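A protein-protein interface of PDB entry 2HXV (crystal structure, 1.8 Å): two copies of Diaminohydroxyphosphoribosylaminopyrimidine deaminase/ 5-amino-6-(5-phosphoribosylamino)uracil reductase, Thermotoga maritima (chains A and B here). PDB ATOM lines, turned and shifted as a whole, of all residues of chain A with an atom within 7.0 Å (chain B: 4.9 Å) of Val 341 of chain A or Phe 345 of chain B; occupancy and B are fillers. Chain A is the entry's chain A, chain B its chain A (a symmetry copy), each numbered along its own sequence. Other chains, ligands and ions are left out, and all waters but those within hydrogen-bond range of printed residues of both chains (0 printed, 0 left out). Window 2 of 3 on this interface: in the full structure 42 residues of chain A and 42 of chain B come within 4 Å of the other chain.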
ATOM      1  N   VAL A 308      20.807  25.513  -3.720  1.00  0.00           N
ATOM      2  CA  VAL A 308      20.835  24.220  -4.381  1.00  0.00           C
ATOM      3  C   VAL A 308      19.674  24.169  -5.353  1.00  0.00           C
ATOM      4  O   VAL A 308      18.624  24.731  -5.095  1.00  0.00           O
ATOM      5  CB  VAL A 308      20.765  23.088  -3.367  1.00  0.00           C
ATOM      6  CG1 VAL A 308      19.461  23.049  -2.620  1.00  0.00           C
ATOM      7  CG2 VAL A 308      21.093  21.731  -4.034  1.00  0.00           C
ATOM      8  N   VAL A 309      19.883  23.494  -6.480  1.00  0.00           N
ATOM      9  CA  VAL A 309      18.841  23.244  -7.449  1.00  0.00           C
ATOM     10  C   VAL A 309      18.735  21.724  -7.640  1.00  0.00           C
ATOM     11  O   VAL A 309      19.738  21.031  -7.813  1.00  0.00           O
ATOM     12  CB  VAL A 309      19.132  23.970  -8.811  1.00  0.00           C
ATOM     13  CG1 VAL A 309      18.026  23.649  -9.834  1.00  0.00           C
ATOM     14  CG2 VAL A 309      19.288  25.439  -8.604  1.00  0.00           C
ATOM     15  N   LYS A 339      27.429  23.764 -10.590  1.00  0.00           N
ATOM     16  CA  LYS A 339      28.072  22.502 -10.797  1.00  0.00           C
ATOM     17  C   LYS A 339      27.197  21.343 -10.381  1.00  0.00           C
ATOM     18  O   LYS A 339      26.463  21.432  -9.418  1.00  0.00           O
ATOM     19  CB  LYS A 339      29.427  22.440 -10.097  1.00  0.00           C
ATOM     20  CG  LYS A 339      29.454  22.654  -8.644  1.00  0.00           C
ATOM     21  N   VAL A 340      27.334  20.227 -11.102  1.00  0.00           N
ATOM     22  CA  VAL A 340      26.604  18.997 -10.780  1.00  0.00           C
ATOM     23  C   VAL A 340      27.313  18.298  -9.640  1.00  0.00           C
ATOM     24  O   VAL A 340      28.542  18.054  -9.701  1.00  0.00           O
ATOM     25  CB  VAL A 340      26.542  18.056 -11.975  1.00  0.00           C
ATOM     26  CG1 VAL A 340      25.785  16.775 -11.632  1.00  0.00           C
ATOM     27  CG2 VAL A 340      25.880  18.746 -13.129  1.00  0.00           C
ATOM     28  N   VAL A 341      26.599  17.986  -8.577  1.00  0.00           N
ATOM     29  CA  VAL A 341      27.264  17.309  -7.461  1.00  0.00           C
ATOM     30  C   VAL A 341      26.756  15.903  -7.303  1.00  0.00           C
ATOM     31  O   VAL A 341      27.383  15.095  -6.663  1.00  0.00           O
ATOM     32  CB  VAL A 341      27.126  18.149  -6.151  1.00  0.00           C
ATOM     33  CG1 VAL A 341      27.725  19.507  -6.373  1.00  0.00           C
ATOM     34  CG2 VAL A 341      25.702  18.283  -5.757  1.00  0.00           C
ATOM     35  N   ASN A 342      25.639  15.590  -7.908  1.00  0.00           N
ATOM     36  CA  ASN A 342      25.086  14.266  -7.809  1.00  0.00           C
ATOM     37  C   ASN A 342      24.031  14.048  -8.874  1.00  0.00           C
ATOM     38  O   ASN A 342      23.338  14.985  -9.269  1.00  0.00           O
ATOM     39  CB  ASN A 342      24.498  14.028  -6.420  1.00  0.00           C
ATOM     40  CG  ASN A 342      24.068  12.580  -6.195  1.00  0.00           C
ATOM     41  OD1 ASN A 342      24.763  11.640  -6.589  1.00  0.00           O
ATOM     42  ND2 ASN A 342      22.906  12.401  -5.579  1.00  0.00           N
ATOM     43  N   VAL A 343      23.946  12.814  -9.372  1.00  0.00           N
ATOM     44  CA  VAL A 343      22.871  12.399 -10.280  1.00  0.00           C
ATOM     45  C   VAL A 343      22.341  11.069  -9.794  1.00  0.00           C
ATOM     46  O   VAL A 343      23.100  10.224  -9.335  1.00  0.00           O
ATOM     47  CB  VAL A 343      23.302  12.338 -11.737  1.00  0.00           C
ATOM     48  CG1 VAL A 343      22.091  12.148 -12.676  1.00  0.00           C
ATOM     49  CG2 VAL A 343      23.942  13.604 -12.125  1.00  0.00           C
ATOM     50  N   GLU A 344      21.036  10.888  -9.816  1.00  0.00           N
ATOM     51  CA  GLU A 344      20.468   9.584  -9.530  1.00  0.00           C
ATOM     52  C   GLU A 344      19.464   9.265 -10.628  1.00  0.00           C
ATOM     53  O   GLU A 344      18.892  10.173 -11.243  1.00  0.00           O
ATOM     54  CB  GLU A 344      19.817   9.607  -8.173  1.00  0.00           C
ATOM     55  CG  GLU A 344      20.898   9.775  -7.066  1.00  0.00           C
ATOM     56  CD  GLU A 344      20.354   9.876  -5.688  1.00  0.00           C
ATOM     57  OE1 GLU A 344      19.119   9.797  -5.530  1.00  0.00           O
ATOM     58  OE2 GLU A 344      21.183  10.034  -4.760  1.00  0.00           O
ATOM     59  N   VAL A 352      19.098  15.468 -10.833  1.00  0.00           N
ATOM     60  CA  VAL A 352      20.384  16.129 -10.861  1.00  0.00           C
ATOM     61  C   VAL A 352      20.390  17.119  -9.720  1.00  0.00           C
ATOM     62  O   VAL A 352      19.481  17.924  -9.627  1.00  0.00           O
ATOM     63  CB  VAL A 352      20.589  16.899 -12.173  1.00  0.00           C
ATOM     64  CG1 VAL A 352      21.991  17.431 -12.294  1.00  0.00           C
ATOM     65  CG2 VAL A 352      20.265  16.000 -13.404  1.00  0.00           C
ATOM     66  N   GLU A 353      21.395  17.044  -8.853  1.00  0.00           N
ATOM     67  CA  GLU A 353      21.600  18.045  -7.807  1.00  0.00           C
ATOM     68  C   GLU A 353      22.717  18.976  -8.247  1.00  0.00           C
ATOM     69  O   GLU A 353      23.802  18.523  -8.606  1.00  0.00           O
ATOM     70  CB  GLU A 353      21.946  17.412  -6.440  1.00  0.00           C
ATOM     71  CG  GLU A 353      22.221  18.502  -5.364  1.00  0.00           C
ATOM     72  CD  GLU A 353      22.613  17.962  -4.005  1.00  0.00           C
ATOM     73  OE1 GLU A 353      22.384  16.777  -3.724  1.00  0.00           O
ATOM     74  OE2 GLU A 353      23.230  18.714  -3.263  1.00  0.00           O
ATOM     75  N   MET A 354      22.426  20.280  -8.236  1.00  0.00           N
ATOM     76  CA  MET A 354      23.370  21.270  -8.665  1.00  0.00           C
ATOM     77  C   MET A 354      23.628  22.310  -7.577  1.00  0.00           C
ATOM     78  O   MET A 354      22.714  22.699  -6.861  1.00  0.00           O
ATOM     79  CB  MET A 354      22.838  21.889  -9.949  1.00  0.00           C
ATOM     80  CG  MET A 354      22.842  20.897 -11.103  1.00  0.00           C
ATOM     81  SD  MET A 354      21.688  21.573 -12.431  1.00  0.00           S
ATOM     82  CE  MET A 354      19.913  20.966 -11.825  1.00  0.00           C
ATOM     83  N   ARG A 355      24.865  22.785  -7.454  1.00  0.00           N
ATOM     84  CA  ARG A 355      25.182  23.775  -6.492  1.00  0.00           C
ATOM     85  C   ARG A 355      25.926  24.922  -7.144  1.00  0.00           C
ATOM     86  O   ARG A 355      26.661  24.719  -8.103  1.00  0.00           O
ATOM     87  CB  ARG A 355      26.092  23.145  -5.473  1.00  0.00           C
ATOM     88  CG  ARG A 355      25.443  21.994  -4.699  1.00  0.00           C
ATOM     89  CD  ARG A 355      24.944  22.461  -3.367  1.00  0.00           C
ATOM     90  NE  ARG A 355      24.189  21.434  -2.660  1.00  0.00           N
ATOM     91  CZ  ARG A 355      23.780  21.573  -1.395  1.00  0.00           C
ATOM     92  NH1 ARG A 355      24.089  22.670  -0.703  1.00  0.00           N
ATOM     93  NH2 ARG A 355      23.074  20.596  -0.818  1.00  0.00           N
ATOM     94  N   PRO A 356      25.722  26.133  -6.626  1.00  0.00           N
ATOM     95  CA  PRO A 356      26.314  27.324  -7.187  1.00  0.00           C
ATOM     96  C   PRO A 356      27.820  27.256  -7.213  1.00  0.00           C
ATOM     97  O   PRO A 356      28.422  26.758  -6.281  1.00  0.00           O
ATOM     98  CB  PRO A 356      25.861  28.426  -6.237  1.00  0.00           C
ATOM     99  CG  PRO A 356      24.731  27.902  -5.475  1.00  0.00           C
ATOM    100  CD  PRO A 356      24.843  26.422  -5.476  1.00  0.00           C
ATOM    101  N   VAL B 343      24.051   7.520 -16.402  1.00  0.00           N
ATOM    102  CA  VAL B 343      24.275   8.966 -16.282  1.00  0.00           C
ATOM    103  C   VAL B 343      25.726   9.182 -15.916  1.00  0.00           C
ATOM    104  O   VAL B 343      26.295   8.419 -15.145  1.00  0.00           O
ATOM    105  CB  VAL B 343      23.335   9.642 -15.296  1.00  0.00           C
ATOM    106  CG1 VAL B 343      23.432  11.180 -15.389  1.00  0.00           C
ATOM    107  CG2 VAL B 343      21.942   9.288 -15.606  1.00  0.00           C
ATOM    108  N   GLU B 344      26.364  10.168 -16.511  1.00  0.00           N
ATOM    109  CA  GLU B 344      27.700  10.545 -16.086  1.00  0.00           C
ATOM    110  C   GLU B 344      27.719  12.054 -15.900  1.00  0.00           C
ATOM    111  O   GLU B 344      26.943  12.778 -16.534  1.00  0.00           O
ATOM    112  CB  GLU B 344      28.699  10.100 -17.121  1.00  0.00           C
ATOM    113  CG  GLU B 344      28.764   8.546 -17.167  1.00  0.00           C
ATOM    114  CD  GLU B 344      29.675   8.000 -18.205  1.00  0.00           C
ATOM    115  OE1 GLU B 344      30.312   8.803 -18.917  1.00  0.00           O
ATOM    116  OE2 GLU B 344      29.748   6.751 -18.298  1.00  0.00           O
ATOM    117  N   PHE B 345      28.580  12.561 -15.038  1.00  0.00           N
ATOM    118  CA  PHE B 345      28.659  14.013 -14.934  1.00  0.00           C
ATOM    119  C   PHE B 345      30.049  14.493 -14.623  1.00  0.00           C
ATOM    120  O   PHE B 345      30.877  13.763 -14.090  1.00  0.00           O
ATOM    121  CB  PHE B 345      27.686  14.562 -13.915  1.00  0.00           C
ATOM    122  CG  PHE B 345      27.949  14.153 -12.505  1.00  0.00           C
ATOM    123  CD1 PHE B 345      27.447  12.954 -12.001  1.00  0.00           C
ATOM    124  CD2 PHE B 345      28.662  14.979 -11.652  1.00  0.00           C
ATOM    125  CE1 PHE B 345      27.651  12.595 -10.738  1.00  0.00           C
ATOM    126  CE2 PHE B 345      28.862  14.604 -10.353  1.00  0.00           C
ATOM    127  CZ  PHE B 345      28.351  13.413  -9.893  1.00  0.00           C
ATOM    128  N   SER B 346      30.278  15.723 -14.983  1.00  0.00           N
ATOM    129  CA  SER B 346      31.531  16.360 -14.647  1.00  0.00           C
ATOM    130  C   SER B 346      31.328  17.852 -14.639  1.00  0.00           C
ATOM    131  O   SER B 346      30.865  18.408 -15.611  1.00  0.00           O
ATOM    132  CB  SER B 346      32.537  16.034 -15.751  1.00  0.00           C
ATOM    133  OG  SER B 346      33.778  16.632 -15.452  1.00  0.00           O
ATOM    134  N   ASP B 347      31.724  18.506 -13.559  1.00  0.00           N
ATOM    135  CA  ASP B 347      31.670  19.934 -13.452  1.00  0.00           C
ATOM    136  C   ASP B 347      30.260  20.452 -13.732  1.00  0.00           C
ATOM    137  O   ASP B 347      29.371  20.187 -12.947  1.00  0.00           O
ATOM    138  CB  ASP B 347      32.742  20.579 -14.346  1.00  0.00           C
ATOM    139  CG  ASP B 347      34.160  20.357 -13.799  1.00  0.00           C
ATOM    140  OD1 ASP B 347      34.312  19.885 -12.646  1.00  0.00           O
ATOM    141  OD2 ASP B 347      35.125  20.662 -14.526  1.00  0.00           O
ATOM    142  N   GLU B 349      28.381  19.755 -16.425  1.00  0.00           N
ATOM    143  CA  GLU B 349      27.774  19.000 -17.480  1.00  0.00           C
ATOM    144  C   GLU B 349      27.384  17.617 -17.006  1.00  0.00           C
ATOM    145  O   GLU B 349      27.978  17.059 -16.085  1.00  0.00           O
ATOM    146  CB  GLU B 349      28.755  18.850 -18.628  1.00  0.00           C
ATOM    147  CG  GLU B 349      28.946  20.150 -19.418  1.00  0.00           C
ATOM    148  CD  GLU B 349      30.179  20.089 -20.259  1.00  0.00           C
ATOM    149  OE1 GLU B 349      30.160  19.343 -21.263  1.00  0.00           O
ATOM    150  OE2 GLU B 349      31.161  20.760 -19.874  1.00  0.00           O
ATOM    151  N   PHE B 350      26.373  17.073 -17.635  1.00  0.00           N
ATOM    152  CA  PHE B 350      25.993  15.690 -17.452  1.00  0.00           C
ATOM    153  C   PHE B 350      25.495  15.031 -18.743  1.00  0.00           C
ATOM    154  O   PHE B 350      25.002  15.676 -19.636  1.00  0.00           O
ATOM    155  CB  PHE B 350      25.008  15.561 -16.269  1.00  0.00           C
ATOM    156  CG  PHE B 350      23.693  16.245 -16.441  1.00  0.00           C
ATOM    157  CD1 PHE B 350      23.510  17.549 -16.001  1.00  0.00           C
ATOM    158  CD2 PHE B 350      22.609  15.558 -16.936  1.00  0.00           C
ATOM    159  CE1 PHE B 350      22.290  18.172 -16.116  1.00  0.00           C
ATOM    160  CE2 PHE B 350      21.380  16.175 -17.086  1.00  0.00           C
ATOM    161  CZ  PHE B 350      21.216  17.490 -16.667  1.00  0.00           C
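N of Val 340 of chain A sits at hydrogen-bond distance from O of Asp 347 of chain B (2.7 Å).
N of Lys 339 of chain A is in hydrogen-bond range of O of Arg 355 of chain A (2.8 Å).
The backbone NH (N) of Val 341 of chain A lies within hydrogen-bond range of the backbone carbonyl oxygen (O) of Glu 353 of chain A (2.8 Å).
The side-chain amide nitrogen of Asn 342 of chain A sits at hydrogen-bond distance from the side-chain carboxylate of Glu 344 of chain A (3.0 Å).
The backbone carbonyl oxygen of Asn 342 of chain A sits at hydrogen-bond distance from the backbone NH of Glu 353 of chain A, at 2.9 Å.
Among the printed residues, pairs that only touch across the chains: Val 343 of chain A with Val 343 of chain B (3.2 Å), Val 340 of chain A with Phe 345 of chain B (3.4 Å), Lys 339 of chain A with Asp 347 of chain B (3.4 Å), Val 343 of chain A with Phe 345 of chain B (3.6 Å), Val 352 of chain A with Phe 350 of chain B (3.7 Å), Val 341 of chain A with Phe 345 of chain B (3.8 Å), Val 340 of chain A with Phe 350 of chain B (3.9 Å), Asn 342 of chain A with Phe 345 of chain B (3.97 Å) and Val 340 of chain A with Glu 349 of chain B (3.998 Å).
Of the printed residues of chain B, Lys 339 of chain A touches Asp 347 (3.4 Å).
Printed residues of chain B within 4 Å of Val 352 of chain A: Phe 350 (3.7 Å).
Arg 355 of chain A touches none of the printed residues of chain B.
Of chain A, only Val 340 (3.4 Å), Val 341 (3.8 Å), Asn 342 (3.97 Å) and Val 343 (3.6 Å) come within 4 Å of Phe 345 of chain B.
Hydrophobic or aromatic side chains of chain B that line the printed part of chain A: Val 343, Phe 345 and Phe 350.
Of the 13 printed residues of chain A, 6 touch a printed residue of chain B.
Hydrophobic or aromatic side chains of chain A within 4 Å of the printed part of chain B: Val 340, Val 343 and Val 352.
Among the printed residues, no Asp or Glu carboxylate lies within 4 Å of a Lys or Arg side-chain nitrogen of the other chain.
Val 343 of chain B touches its own counterpart, Val 343 of chain A.
Positions printed for both chains: 343 and 344.
Of the 10 pairs that touch across the chains among the printed residues, 1 has its exchanged pair printed and touching as well.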
